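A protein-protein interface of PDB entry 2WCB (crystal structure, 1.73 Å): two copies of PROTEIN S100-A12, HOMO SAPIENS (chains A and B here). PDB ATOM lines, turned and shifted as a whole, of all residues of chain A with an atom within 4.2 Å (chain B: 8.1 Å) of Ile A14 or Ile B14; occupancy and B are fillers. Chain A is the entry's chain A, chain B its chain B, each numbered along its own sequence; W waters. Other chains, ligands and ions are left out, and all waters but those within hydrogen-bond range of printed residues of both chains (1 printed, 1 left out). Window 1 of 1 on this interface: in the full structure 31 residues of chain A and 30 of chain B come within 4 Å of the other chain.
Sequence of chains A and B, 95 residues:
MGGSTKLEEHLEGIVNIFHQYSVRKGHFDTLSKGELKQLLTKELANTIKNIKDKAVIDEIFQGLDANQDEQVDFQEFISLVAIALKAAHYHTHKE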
ATOM      1  N   HIS A  10       6.677 -25.317  21.668  1.00  0.00           N
ATOM      2  CA  HIS A  10       6.599 -23.977  22.189  1.00  0.00           C
ATOM      3  C   HIS A  10       7.687 -23.101  21.533  1.00  0.00           C
ATOM      4  O   HIS A  10       7.475 -21.981  21.123  1.00  0.00           O
ATOM      5  CB  HIS A  10       6.717 -23.970  23.703  1.00  0.00           C
ATOM      6  CG  HIS A  10       5.591 -24.682  24.387  1.00  0.00           C
ATOM      7  ND1 HIS A  10       4.264 -24.393  24.157  1.00  0.00           N
ATOM      8  CD2 HIS A  10       5.613 -25.626  25.352  1.00  0.00           C
ATOM      9  CE1 HIS A  10       3.523 -25.204  24.907  1.00  0.00           C
ATOM     10  NE2 HIS A  10       4.325 -25.931  25.662  1.00  0.00           N
ATOM     11  N   LEU A  11       8.853 -23.655  21.289  1.00  0.00           N
ATOM     12  CA  LEU A  11       9.840 -22.819  20.643  1.00  0.00           C
ATOM     13  C   LEU A  11       9.411 -22.481  19.209  1.00  0.00           C
ATOM     14  O   LEU A  11       9.555 -21.335  18.743  1.00  0.00           O
ATOM     15  CB  LEU A  11      11.197 -23.567  20.613  1.00  0.00           C
ATOM     16  CG  LEU A  11      11.656 -23.880  22.037  1.00  0.00           C
ATOM     17  CD1 LEU A  11      13.023 -24.489  21.904  1.00  0.00           C
ATOM     18  CD2 LEU A  11      11.577 -22.647  23.024  1.00  0.00           C
ATOM     19  N   GLU A  12       8.875 -23.501  18.547  1.00  0.00           N
ATOM     20  CA  GLU A  12       8.397 -23.459  17.188  1.00  0.00           C
ATOM     21  C   GLU A  12       7.319 -22.397  17.042  1.00  0.00           C
ATOM     22  O   GLU A  12       7.241 -21.695  16.038  1.00  0.00           O
ATOM     23  CB  GLU A  12       7.839 -24.839  16.813  1.00  0.00           C
ATOM     24  CG  GLU A  12       8.950 -25.789  16.356  1.00  0.00           C
ATOM     25  CD  GLU A  12       8.581 -27.268  16.311  1.00  0.00           C
ATOM     26  OE1 GLU A  12       7.380 -27.633  16.337  1.00  0.00           O
ATOM     27  OE2 GLU A  12       9.516 -28.077  16.220  1.00  0.00           O
ATOM     28  N   GLY A  13       6.486 -22.329  18.060  1.00  0.00           N
ATOM     29  CA  GLY A  13       5.320 -21.467  18.089  1.00  0.00           C
ATOM     30  C   GLY A  13       5.705 -20.016  18.260  1.00  0.00           C
ATOM     31  O   GLY A  13       5.130 -19.152  17.602  1.00  0.00           O
ATOM     32  N   ILE A  14       6.705 -19.766  19.105  1.00  0.00           N
ATOM     33  CA  ILE A  14       7.200 -18.459  19.384  1.00  0.00           C
ATOM     34  C   ILE A  14       7.852 -17.905  18.073  1.00  0.00           C
ATOM     35  O   ILE A  14       7.650 -16.741  17.674  1.00  0.00           O
ATOM     36  CB  ILE A  14       8.204 -18.423  20.577  1.00  0.00           C
ATOM     37  CG1 ILE A  14       7.534 -18.839  21.936  1.00  0.00           C
ATOM     38  CG2 ILE A  14       8.822 -17.018  20.690  1.00  0.00           C
ATOM     39  CD1 ILE A  14       8.426 -19.051  23.110  1.00  0.00           C
ATOM     40  N   VAL A  15       8.630 -18.746  17.415  1.00  0.00           N
ATOM     41  CA  VAL A  15       9.182 -18.381  16.097  1.00  0.00           C
ATOM     42  C   VAL A  15       8.125 -18.087  15.064  1.00  0.00           C
ATOM     43  O   VAL A  15       8.228 -17.106  14.306  1.00  0.00           O
ATOM     44  CB  VAL A  15      10.111 -19.473  15.502  1.00  0.00           C
ATOM     45  CG1 VAL A  15      10.484 -19.119  14.035  1.00  0.00           C
ATOM     46  CG2 VAL A  15      11.347 -19.656  16.354  1.00  0.00           C
ATOM     47  N   ASN A  16       7.060 -18.879  15.066  1.00  0.00           N
ATOM     48  CA  ASN A  16       5.942 -18.644  14.179  1.00  0.00           C
ATOM     49  C   ASN A  16       5.290 -17.288  14.419  1.00  0.00           C
ATOM     50  O   ASN A  16       5.048 -16.533  13.459  1.00  0.00           O
ATOM     51  CB  ASN A  16       4.964 -19.797  14.283  1.00  0.00           C
ATOM     52  CG  ASN A  16       3.784 -19.656  13.371  1.00  0.00           C
ATOM     53  OD1 ASN A  16       3.740 -20.240  12.266  1.00  0.00           O
ATOM     54  ND2 ASN A  16       2.787 -18.919  13.830  1.00  0.00           N
ATOM     55  N   ILE A  17       4.990 -16.981  15.690  1.00  0.00           N
ATOM     56  CA  ILE A  17       4.435 -15.710  16.033  1.00  0.00           C
ATOM     57  C   ILE A  17       5.299 -14.542  15.565  1.00  0.00           C
ATOM     58  O   ILE A  17       4.807 -13.642  14.929  1.00  0.00           O
ATOM     59  CB  ILE A  17       4.058 -15.584  17.524  1.00  0.00           C
ATOM     60  CG1 ILE A  17       2.844 -16.497  17.872  1.00  0.00           C
ATOM     61  CG2 ILE A  17       3.650 -14.183  17.814  1.00  0.00           C
ATOM     62  CD1 ILE A  17       2.836 -17.030  19.311  1.00  0.00           C
ATOM     63  N   PHE A  18       6.582 -14.569  15.854  1.00  0.00           N
ATOM     64  CA  PHE A  18       7.503 -13.563  15.344  1.00  0.00           C
ATOM     65  C   PHE A  18       7.351 -13.384  13.841  1.00  0.00           C
ATOM     66  O   PHE A  18       7.191 -12.251  13.349  1.00  0.00           O
ATOM     67  CB  PHE A  18       8.964 -13.930  15.692  1.00  0.00           C
ATOM     68  CG  PHE A  18       9.995 -12.973  15.090  1.00  0.00           C
ATOM     69  CD1 PHE A  18      10.321 -11.777  15.723  1.00  0.00           C
ATOM     70  CD2 PHE A  18      10.641 -13.279  13.889  1.00  0.00           C
ATOM     71  CE1 PHE A  18      11.287 -10.877  15.131  1.00  0.00           C
ATOM     72  CE2 PHE A  18      11.586 -12.408  13.307  1.00  0.00           C
ATOM     73  CZ  PHE A  18      11.925 -11.223  13.930  1.00  0.00           C
ATOM     74  N   PHE A  77      14.166  -9.810  19.705  1.00  0.00           N
ATOM     75  CA  PHE A  77      12.926 -10.414  20.132  1.00  0.00           C
ATOM     76  C   PHE A  77      13.131 -11.503  21.217  1.00  0.00           C
ATOM     77  O   PHE A  77      12.392 -11.500  22.180  1.00  0.00           O
ATOM     78  CB  PHE A  77      12.147 -10.948  18.949  1.00  0.00           C
ATOM     79  CG  PHE A  77      10.827 -11.578  19.307  1.00  0.00           C
ATOM     80  CD1 PHE A  77      10.661 -12.930  19.213  1.00  0.00           C
ATOM     81  CD2 PHE A  77       9.743 -10.807  19.665  1.00  0.00           C
ATOM     82  CE1 PHE A  77       9.487 -13.509  19.493  1.00  0.00           C
ATOM     83  CE2 PHE A  77       8.560 -11.391  19.969  1.00  0.00           C
ATOM     84  CZ  PHE A  77       8.423 -12.730  19.896  1.00  0.00           C
ATOM     85  N   VAL A  81      11.450 -11.996  24.898  1.00  0.00           N
ATOM     86  CA  VAL A  81      10.844 -13.265  25.295  1.00  0.00           C
ATOM     87  C   VAL A  81      11.387 -13.687  26.686  1.00  0.00           C
ATOM     88  O   VAL A  81      10.631 -14.113  27.540  1.00  0.00           O
ATOM     89  CB  VAL A  81      10.993 -14.332  24.218  1.00  0.00           C
ATOM     90  CG1 VAL A  81      10.696 -15.699  24.770  1.00  0.00           C
ATOM     91  CG2 VAL A  81      10.023 -13.991  23.018  1.00  0.00           C
ATOM     92  N   LEU A  85       9.230 -14.361  29.926  1.00  0.00           N
ATOM     93  CA  LEU A  85       9.278 -15.680  30.548  1.00  0.00           C
ATOM     94  C   LEU A  85       9.471 -15.540  32.073  1.00  0.00           C
ATOM     95  O   LEU A  85       8.810 -16.250  32.851  1.00  0.00           O
ATOM     96  CB  LEU A  85      10.463 -16.487  29.966  1.00  0.00           C
ATOM     97  CG  LEU A  85      10.053 -17.441  28.872  1.00  0.00           C
ATOM     98  CD1 LEU A  85      11.295 -18.005  28.183  1.00  0.00           C
ATOM     99  CD2 LEU A  85       9.138 -18.566  29.533  1.00  0.00           C
ATOM    100  N   LYS B   6      -1.910 -17.049  22.048  1.00  0.00           N
ATOM    101  CA  LYS B   6      -0.996 -18.174  21.737  1.00  0.00           C
ATOM    102  C   LYS B   6       0.442 -17.967  22.264  1.00  0.00           C
ATOM    103  O   LYS B   6       1.062 -18.892  22.829  1.00  0.00           O
ATOM    104  CB  LYS B   6      -1.016 -18.502  20.254  1.00  0.00           C
ATOM    105  CG  LYS B   6      -2.285 -19.293  19.820  1.00  0.00           C
ATOM    106  CD  LYS B   6      -2.483 -19.428  18.342  1.00  0.00           C
ATOM    107  CE  LYS B   6      -3.822 -20.104  18.005  1.00  0.00           C
ATOM    108  NZ  LYS B   6      -4.181 -19.923  16.570  1.00  0.00           N
ATOM    109  N   LEU B   7       0.967 -16.757  22.085  1.00  0.00           N
ATOM    110  CA  LEU B   7       2.229 -16.415  22.688  1.00  0.00           C
ATOM    111  C   LEU B   7       2.189 -16.573  24.205  1.00  0.00           C
ATOM    112  O   LEU B   7       3.079 -17.136  24.744  1.00  0.00           O
ATOM    113  CB  LEU B   7       2.668 -15.001  22.316  1.00  0.00           C
ATOM    114  CG  LEU B   7       4.052 -14.628  22.885  1.00  0.00           C
ATOM    115  CD1 LEU B   7       5.120 -15.584  22.383  1.00  0.00           C
ATOM    116  CD2 LEU B   7       4.397 -13.090  22.592  1.00  0.00           C
ATOM    117  N   GLU B   8       1.161 -16.122  24.941  1.00  0.00           N
ATOM    118  CA  GLU B   8       1.170 -16.329  26.367  1.00  0.00           C
ATOM    119  C   GLU B   8       1.065 -17.826  26.777  1.00  0.00           C
ATOM    120  O   GLU B   8       1.555 -18.232  27.813  1.00  0.00           O
ATOM    121  CB  GLU B   8       0.040 -15.504  27.006  1.00  0.00           C
ATOM    122  CG  GLU B   8       0.318 -14.051  26.661  1.00  0.00           C
ATOM    123  CD  GLU B   8      -0.834 -13.236  27.072  1.00  0.00           C
ATOM    124  OE1 GLU B   8      -1.824 -13.914  27.109  1.00  0.00           O
ATOM    125  OE2 GLU B   8      -0.687 -12.082  27.422  1.00  0.00           O
ATOM    126  N   GLU B   9       0.400 -18.623  25.953  1.00  0.00           N
ATOM    127  CA  GLU B   9       0.229 -20.035  26.227  1.00  0.00           C
ATOM    128  C   GLU B   9       1.628 -20.721  26.074  1.00  0.00           C
ATOM    129  O   GLU B   9       1.948 -21.608  26.861  1.00  0.00           O
ATOM    130  CB  GLU B   9      -0.676 -20.632  25.207  1.00  0.00           C
ATOM    131  CG  GLU B   9      -2.145 -20.322  25.464  1.00  0.00           C
ATOM    132  CD  GLU B   9      -3.038 -20.755  24.304  1.00  0.00           C
ATOM    133  OE1 GLU B   9      -2.549 -21.391  23.335  1.00  0.00           O
ATOM    134  OE2 GLU B   9      -4.244 -20.451  24.350  1.00  0.00           O
ATOM    135  N   HIS B  10       2.383 -20.302  25.104  1.00  0.00           N
ATOM    136  CA  HIS B  10       3.751 -20.866  24.913  1.00  0.00           C
ATOM    137  C   HIS B  10       4.653 -20.550  26.071  1.00  0.00           C
ATOM    138  O   HIS B  10       5.470 -21.457  26.508  1.00  0.00           O
ATOM    139  CB  HIS B  10       4.456 -20.394  23.648  1.00  0.00           C
ATOM    140  CG  HIS B  10       3.837 -20.893  22.408  1.00  0.00           C
ATOM    141  ND1 HIS B  10       3.430 -22.205  22.259  1.00  0.00           N
ATOM    142  CD2 HIS B  10       3.581 -20.278  21.242  1.00  0.00           C
ATOM    143  CE1 HIS B  10       2.915 -22.352  21.053  1.00  0.00           C
ATOM    144  NE2 HIS B  10       2.991 -21.196  20.421  1.00  0.00           N
ATOM    145  N   LEU B  11       4.601 -19.297  26.544  1.00  0.00           N
ATOM    146  CA  LEU B  11       5.383 -18.926  27.739  1.00  0.00           C
ATOM    147  C   LEU B  11       4.990 -19.812  28.945  1.00  0.00           C
ATOM    148  O   LEU B  11       5.861 -20.362  29.634  1.00  0.00           O
ATOM    149  CB  LEU B  11       5.258 -17.428  28.050  1.00  0.00           C
ATOM    150  CG  LEU B  11       5.689 -16.400  27.014  1.00  0.00           C
ATOM    151  CD1 LEU B  11       5.619 -14.954  27.569  1.00  0.00           C
ATOM    152  CD2 LEU B  11       7.119 -16.710  26.490  1.00  0.00           C
ATOM    153  N   GLU B  12       3.688 -19.890  29.270  1.00  0.00           N
ATOM    154  CA  GLU B  12       3.208 -20.754  30.311  1.00  0.00           C
ATOM    155  C   GLU B  12       3.669 -22.229  30.140  1.00  0.00           C
ATOM    156  O   GLU B  12       3.964 -22.888  31.166  1.00  0.00           O
ATOM    157  CB  GLU B  12       1.680 -20.643  30.447  1.00  0.00           C
ATOM    158  CG  GLU B  12       1.102 -21.465  31.553  1.00  0.00           C
ATOM    159  CD  GLU B  12      -0.350 -21.111  31.977  1.00  0.00           C
ATOM    160  OE1 GLU B  12      -0.913 -21.919  32.731  1.00  0.00           O
ATOM    161  OE2 GLU B  12      -0.939 -20.066  31.561  1.00  0.00           O
ATOM    162  N   GLY B  13       3.807 -22.664  28.884  1.00  0.00           N
ATOM    163  CA  GLY B  13       4.052 -24.046  28.479  1.00  0.00           C
ATOM    164  C   GLY B  13       5.495 -24.381  28.844  1.00  0.00           C
ATOM    165  O   GLY B  13       5.758 -25.424  29.410  1.00  0.00           O
ATOM    166  N   ILE B  14       6.355 -23.407  28.629  1.00  0.00           N
ATOM    167  CA  ILE B  14       7.776 -23.473  28.970  1.00  0.00           C
ATOM    168  C   ILE B  14       7.976 -23.478  30.482  1.00  0.00           C
ATOM    169  O   ILE B  14       8.716 -24.302  31.048  1.00  0.00           O
ATOM    170  CB  ILE B  14       8.524 -22.318  28.288  1.00  0.00           C
ATOM    171  CG1 ILE B  14       8.421 -22.420  26.760  1.00  0.00           C
ATOM    172  CG2 ILE B  14      10.012 -22.227  28.796  1.00  0.00           C
ATOM    173  CD1 ILE B  14       8.705 -21.086  26.030  1.00  0.00           C
ATOM    174  N   VAL B  15       7.271 -22.605  31.198  1.00  0.00           N
ATOM    175  CA  VAL B  15       7.255 -22.668  32.648  1.00  0.00           C
ATOM    176  C   VAL B  15       6.807 -24.054  33.142  1.00  0.00           C
ATOM    177  O   VAL B  15       7.451 -24.630  34.040  1.00  0.00           O
ATOM    178  CB  VAL B  15       6.378 -21.571  33.280  1.00  0.00           C
ATOM    179  CG1 VAL B  15       6.328 -21.776  34.815  1.00  0.00           C
ATOM    180  CG2 VAL B  15       6.890 -20.124  32.907  1.00  0.00           C
ATOM    181  N   ASN B  16       5.717 -24.566  32.565  1.00  0.00           N
ATOM    182  CA  ASN B  16       5.111 -25.834  32.900  1.00  0.00           C
ATOM    183  C   ASN B  16       6.084 -26.990  32.796  1.00  0.00           C
ATOM    184  O   ASN B  16       6.138 -27.842  33.750  1.00  0.00           O
ATOM    185  CB  ASN B  16       3.895 -26.122  32.075  1.00  0.00           C
ATOM    186  CG  ASN B  16       2.645 -25.419  32.593  1.00  0.00           C
ATOM    187  OD1 ASN B  16       2.642 -24.830  33.667  1.00  0.00           O
ATOM    188  ND2 ASN B  16       1.636 -25.418  31.778  1.00  0.00           N
ATOM    189  N   ILE B  17       6.928 -26.921  31.765  1.00  0.00           N
ATOM    190  CA  ILE B  17       7.901 -27.998  31.489  1.00  0.00           C
ATOM    191  C   ILE B  17       9.023 -27.938  32.525  1.00  0.00           C
ATOM    192  O   ILE B  17       9.412 -28.998  33.092  1.00  0.00           O
ATOM    193  CB  ILE B  17       8.408 -28.019  30.054  1.00  0.00           C
ATOM    194  CG1 ILE B  17       7.307 -28.548  29.095  1.00  0.00           C
ATOM    195  CG2 ILE B  17       9.664 -28.933  29.883  1.00  0.00           C
ATOM    196  CD1 ILE B  17       7.513 -28.233  27.649  1.00  0.00           C
ATOM    197  N   PHE B  18       9.514 -26.746  32.792  1.00  0.00           N
ATOM    198  CA  PHE B  18      10.438 -26.574  33.912  1.00  0.00           C
ATOM    199  C   PHE B  18       9.938 -27.169  35.215  1.00  0.00           C
ATOM    200  O   PHE B  18      10.642 -27.942  35.865  1.00  0.00           O
ATOM    201  CB  PHE B  18      10.861 -25.122  34.087  1.00  0.00           C
ATOM    202  CG  PHE B  18      11.806 -24.889  35.265  1.00  0.00           C
ATOM    203  CD1 PHE B  18      13.180 -24.946  35.091  1.00  0.00           C
ATOM    204  CD2 PHE B  18      11.315 -24.618  36.546  1.00  0.00           C
ATOM    205  CE1 PHE B  18      14.061 -24.729  36.177  1.00  0.00           C
ATOM    206  CE2 PHE B  18      12.192 -24.397  37.635  1.00  0.00           C
ATOM    207  CZ  PHE B  18      13.567 -24.407  37.419  1.00  0.00           C
ATOM    208  N   HIS B  19       8.703 -26.838  35.584  1.00  0.00           N
ATOM    209  CA  HIS B  19       8.120 -27.249  36.808  1.00  0.00           C
ATOM    210  C   HIS B  19       7.883 -28.755  36.922  1.00  0.00           C
ATOM    211  O   HIS B  19       8.053 -29.335  38.015  1.00  0.00           O
ATOM    212  CB  HIS B  19       6.818 -26.516  37.013  1.00  0.00           C
ATOM    213  CG  HIS B  19       6.969 -25.124  37.551  1.00  0.00           C
ATOM    214  ND1 HIS B  19       5.972 -24.189  37.380  1.00  0.00           N
ATOM    215  CD2 HIS B  19       7.936 -24.516  38.291  1.00  0.00           C
ATOM    216  CE1 HIS B  19       6.322 -23.062  37.973  1.00  0.00           C
ATOM    217  NE2 HIS B  19       7.493 -23.243  38.562  1.00  0.00           N
ATOM    218  N   GLN B  20       7.500 -29.413  35.830  1.00  0.00           N
ATOM    219  CA  GLN B  20       7.269 -30.870  35.872  1.00  0.00           C
ATOM    220  C   GLN B  20       8.575 -31.643  36.129  1.00  0.00           C
ATOM    221  O   GLN B  20       8.525 -32.849  36.448  1.00  0.00           O
ATOM    222  CB  GLN B  20       6.630 -31.364  34.589  1.00  0.00           C
ATOM    223  CG  GLN B  20       7.639 -31.642  33.472  1.00  0.00           C
ATOM    224  CD  GLN B  20       7.040 -31.632  32.080  1.00  0.00           C
ATOM    225  OE1 GLN B  20       6.060 -30.908  31.780  1.00  0.00           O
ATOM    226  NE2 GLN B  20       7.666 -32.400  31.191  1.00  0.00           N
ATOM    227  N   LEU B  39      16.812 -33.155  31.333  1.00  0.00           N
ATOM    228  CA  LEU B  39      15.834 -32.304  30.683  1.00  0.00           C
ATOM    229  C   LEU B  39      16.252 -31.872  29.254  1.00  0.00           C
ATOM    230  O   LEU B  39      15.503 -32.070  28.268  1.00  0.00           O
ATOM    231  CB  LEU B  39      15.514 -31.067  31.546  1.00  0.00           C
ATOM    232  CG  LEU B  39      14.385 -30.138  31.131  1.00  0.00           C
ATOM    233  CD1 LEU B  39      13.927 -29.254  32.380  1.00  0.00           C
ATOM    234  CD2 LEU B  39      14.721 -29.274  29.907  1.00  0.00           C
ATOM    235  N   PHE B  74      15.097 -21.016  37.631  1.00  0.00           N
ATOM    236  CA  PHE B  74      14.436 -20.754  36.410  1.00  0.00           C
ATOM    237  C   PHE B  74      15.209 -19.694  35.566  1.00  0.00           C
ATOM    238  O   PHE B  74      15.293 -19.824  34.331  1.00  0.00           O
ATOM    239  CB  PHE B  74      13.002 -20.311  36.672  1.00  0.00           C
ATOM    240  CG  PHE B  74      12.208 -20.187  35.432  1.00  0.00           C
ATOM    241  CD1 PHE B  74      11.893 -21.344  34.692  1.00  0.00           C
ATOM    242  CD2 PHE B  74      11.741 -18.932  34.982  1.00  0.00           C
ATOM    243  CE1 PHE B  74      11.179 -21.236  33.525  1.00  0.00           C
ATOM    244  CE2 PHE B  74      11.033 -18.848  33.855  1.00  0.00           C
ATOM    245  CZ  PHE B  74      10.709 -19.979  33.121  1.00  0.00           C
ATOM    246  N   PHE B  77      17.526 -21.274  33.583  1.00  0.00           N
ATOM    247  CA  PHE B  77      16.823 -22.030  32.564  1.00  0.00           C
ATOM    248  C   PHE B  77      16.444 -21.114  31.400  1.00  0.00           C
ATOM    249  O   PHE B  77      16.550 -21.528  30.269  1.00  0.00           O
ATOM    250  CB  PHE B  77      15.633 -22.791  33.148  1.00  0.00           C
ATOM    251  CG  PHE B  77      14.877 -23.647  32.162  1.00  0.00           C
ATOM    252  CD1 PHE B  77      13.580 -23.370  31.827  1.00  0.00           C
ATOM    253  CD2 PHE B  77      15.439 -24.746  31.630  1.00  0.00           C
ATOM    254  CE1 PHE B  77      12.875 -24.193  30.966  1.00  0.00           C
ATOM    255  CE2 PHE B  77      14.705 -25.547  30.752  1.00  0.00           C
ATOM    256  CZ  PHE B  77      13.454 -25.254  30.434  1.00  0.00           C
ATOM    257  N   ILE B  78      15.920 -19.918  31.693  1.00  0.00           N
ATOM    258  CA  ILE B  78      15.608 -18.894  30.669  1.00  0.00           C
ATOM    259  C   ILE B  78      16.798 -18.692  29.705  1.00  0.00           C
ATOM    260  O   ILE B  78      16.613 -18.610  28.484  1.00  0.00           O
ATOM    261  CB  ILE B  78      15.177 -17.586  31.317  1.00  0.00           C
ATOM    262  CG1 ILE B  78      13.793 -17.735  31.937  1.00  0.00           C
ATOM    263  CG2 ILE B  78      15.154 -16.416  30.296  1.00  0.00           C
ATOM    264  CD1 ILE B  78      13.507 -16.670  32.832  1.00  0.00           C
ATOM    265  N   VAL B  81      16.816 -21.583  27.436  1.00  0.00           N
ATOM    266  CA  VAL B  81      15.816 -21.457  26.507  1.00  0.00           C
ATOM    267  C   VAL B  81      16.170 -20.460  25.367  1.00  0.00           C
ATOM    268  O   VAL B  81      15.819 -20.700  24.207  1.00  0.00           O
ATOM    269  CB  VAL B  81      14.498 -21.054  27.215  1.00  0.00           C
ATOM    270  CG1 VAL B  81      13.483 -20.688  26.201  1.00  0.00           C
ATOM    271  CG2 VAL B  81      14.005 -22.276  28.112  1.00  0.00           C
ATOM    272  N   ALA B  82      16.870 -19.367  25.696  1.00  0.00           N
ATOM    273  CA  ALA B  82      17.168 -18.283  24.740  1.00  0.00           C
ATOM    274  C   ALA B  82      18.043 -18.809  23.668  1.00  0.00           C
ATOM    275  O   ALA B  82      17.868 -18.471  22.496  1.00  0.00           O
ATOM    276  CB  ALA B  82      17.868 -17.039  25.435  1.00  0.00           C
ATOM    277  N   LEU B  85      16.039 -21.107  21.454  1.00  0.00           N
ATOM    278  CA  LEU B  85      15.117 -20.394  20.633  1.00  0.00           C
ATOM    279  C   LEU B  85      15.792 -19.829  19.390  1.00  0.00           C
ATOM    280  O   LEU B  85      15.143 -19.811  18.325  1.00  0.00           O
ATOM    281  CB  LEU B  85      14.432 -19.308  21.458  1.00  0.00           C
ATOM    282  CG  LEU B  85      13.189 -18.575  20.953  1.00  0.00           C
ATOM    283  CD1 LEU B  85      12.015 -19.595  20.679  1.00  0.00           C
ATOM    284  CD2 LEU B  85      12.801 -17.568  21.987  1.00  0.00           C
ATOM    285  N   HIS B  89      15.130 -21.030  15.523  1.00  0.00           N
ATOM    286  CA  HIS B  89      14.828 -20.020  14.484  1.00  0.00           C
ATOM    287  C   HIS B  89      15.690 -20.324  13.317  1.00  0.00           C
ATOM    288  O   HIS B  89      15.285 -20.471  12.162  1.00  0.00           O
ATOM    289  CB  HIS B  89      14.981 -18.572  15.005  1.00  0.00           C
ATOM    290  CG  HIS B  89      14.762 -17.522  13.945  1.00  0.00           C
ATOM    291  ND1 HIS B  89      15.779 -16.741  13.462  1.00  0.00           N
ATOM    292  CD2 HIS B  89      13.649 -17.157  13.251  1.00  0.00           C
ATOM    293  CE1 HIS B  89      15.333 -15.957  12.496  1.00  0.00           C
ATOM    294  NE2 HIS B  89      14.031 -16.168  12.358  1.00  0.00           N
HETATM  295  O   HOH W   1       0.872 -24.013  23.560  1.00  0.00           O
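A ring nitrogen (ND1) of His B10 sits at hydrogen-bond distance from a ring nitrogen (ND1) of His A10, at 3.0 Å.
Of the 23 printed residues of chain B, 11 touch a printed residue of chain A. Hydrophobic or aromatic side chains of chain B within 4 Å of the printed part of chain A: Leu B7, His B10, Leu B11, Ile B14, Ile B17, Phe B74, Val B81, Leu B85 and His B89. Along chain B the printed residues that touch a printed residue of chain A span positions 6 to 89. Printed residues of chain A that touch a printed residue of chain B: His A10, Leu A11, Gly A13, Ile A14, Val A15, Ile A17, Val A81 and Leu A85. Hydrophobic or aromatic side chains of chain A that line the printed part of chain B: His A10, Leu A11, Ile A14, Val A15, Ile A17, Val A81 and Leu A85. Among the printed residues, 18 pairs touch across the chains.
Of the printed residues of chain B, Ile A14 touches His B10 (3.8 Å), Ile B14 (3.6 Å) and Leu B85 (3.99 Å). Of chain A, only His A10, Ile A14 and Leu A85 come within 4 Å of Ile B14. Of the printed residues of chain A, Phe B74 touches Leu A85. Of the printed residues of chain A, Lys B6 touches Ile A17. Glu A12 touches none of the printed residues of chain B. The nearest printed residue of chain B that does not touch Ile A14 is Leu B7 (4.1 Å). The nearest printed residue of chain A that does not touch Ile B14 is Leu A11 (4.4 Å). The nearest printed residue of chain A that does not touch His B10 is Leu A85 (5.6 Å).
Water W1 bridges a ring nitrogen (ND1) of His B10 (3.4 Å) and a ring nitrogen (ND1) of His A10 (3.5 Å).
Among the printed residues, merely in contact across the chains: His A10 with Gly B13 (3.4 Å), His A10 with Ile B14 (3.8 Å), His A10 with Ile B17 (3.96 Å), Leu A11 with Leu B85 (3.6 Å), Gly A13 with His B10 (3.3 Å), Ile A14 with His B10 (3.8 Å), Ile A14 with Ile B14 (3.6 Å), Ile A14 with Leu B85 (3.99 Å), Val A15 with His B89 (3.8 Å), Ile A17 with Lys B6 (3.9 Å), Ile A17 with Leu B7 (3.4 Å), Ile A17 with His B10 (3.9 Å), Val A81 with Leu B85 (3.96 Å), Leu A85 with Leu B11 (3.7 Å), Leu A85 with Ile B14 (3.8 Å), Leu A85 with Phe B74 (3.6 Å) and Leu A85 with Val B81 (3.99 Å).
His A10 touches its own counterpart, His B10. His A10 touches Gly B13, and with the chains exchanged Gly A13 touches His B10. His A10 touches Ile B14, and with the chains exchanged Ile A14 touches His B10. Leu A11 touches Leu B85, and with the chains exchanged Leu A85 touches Leu B11.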
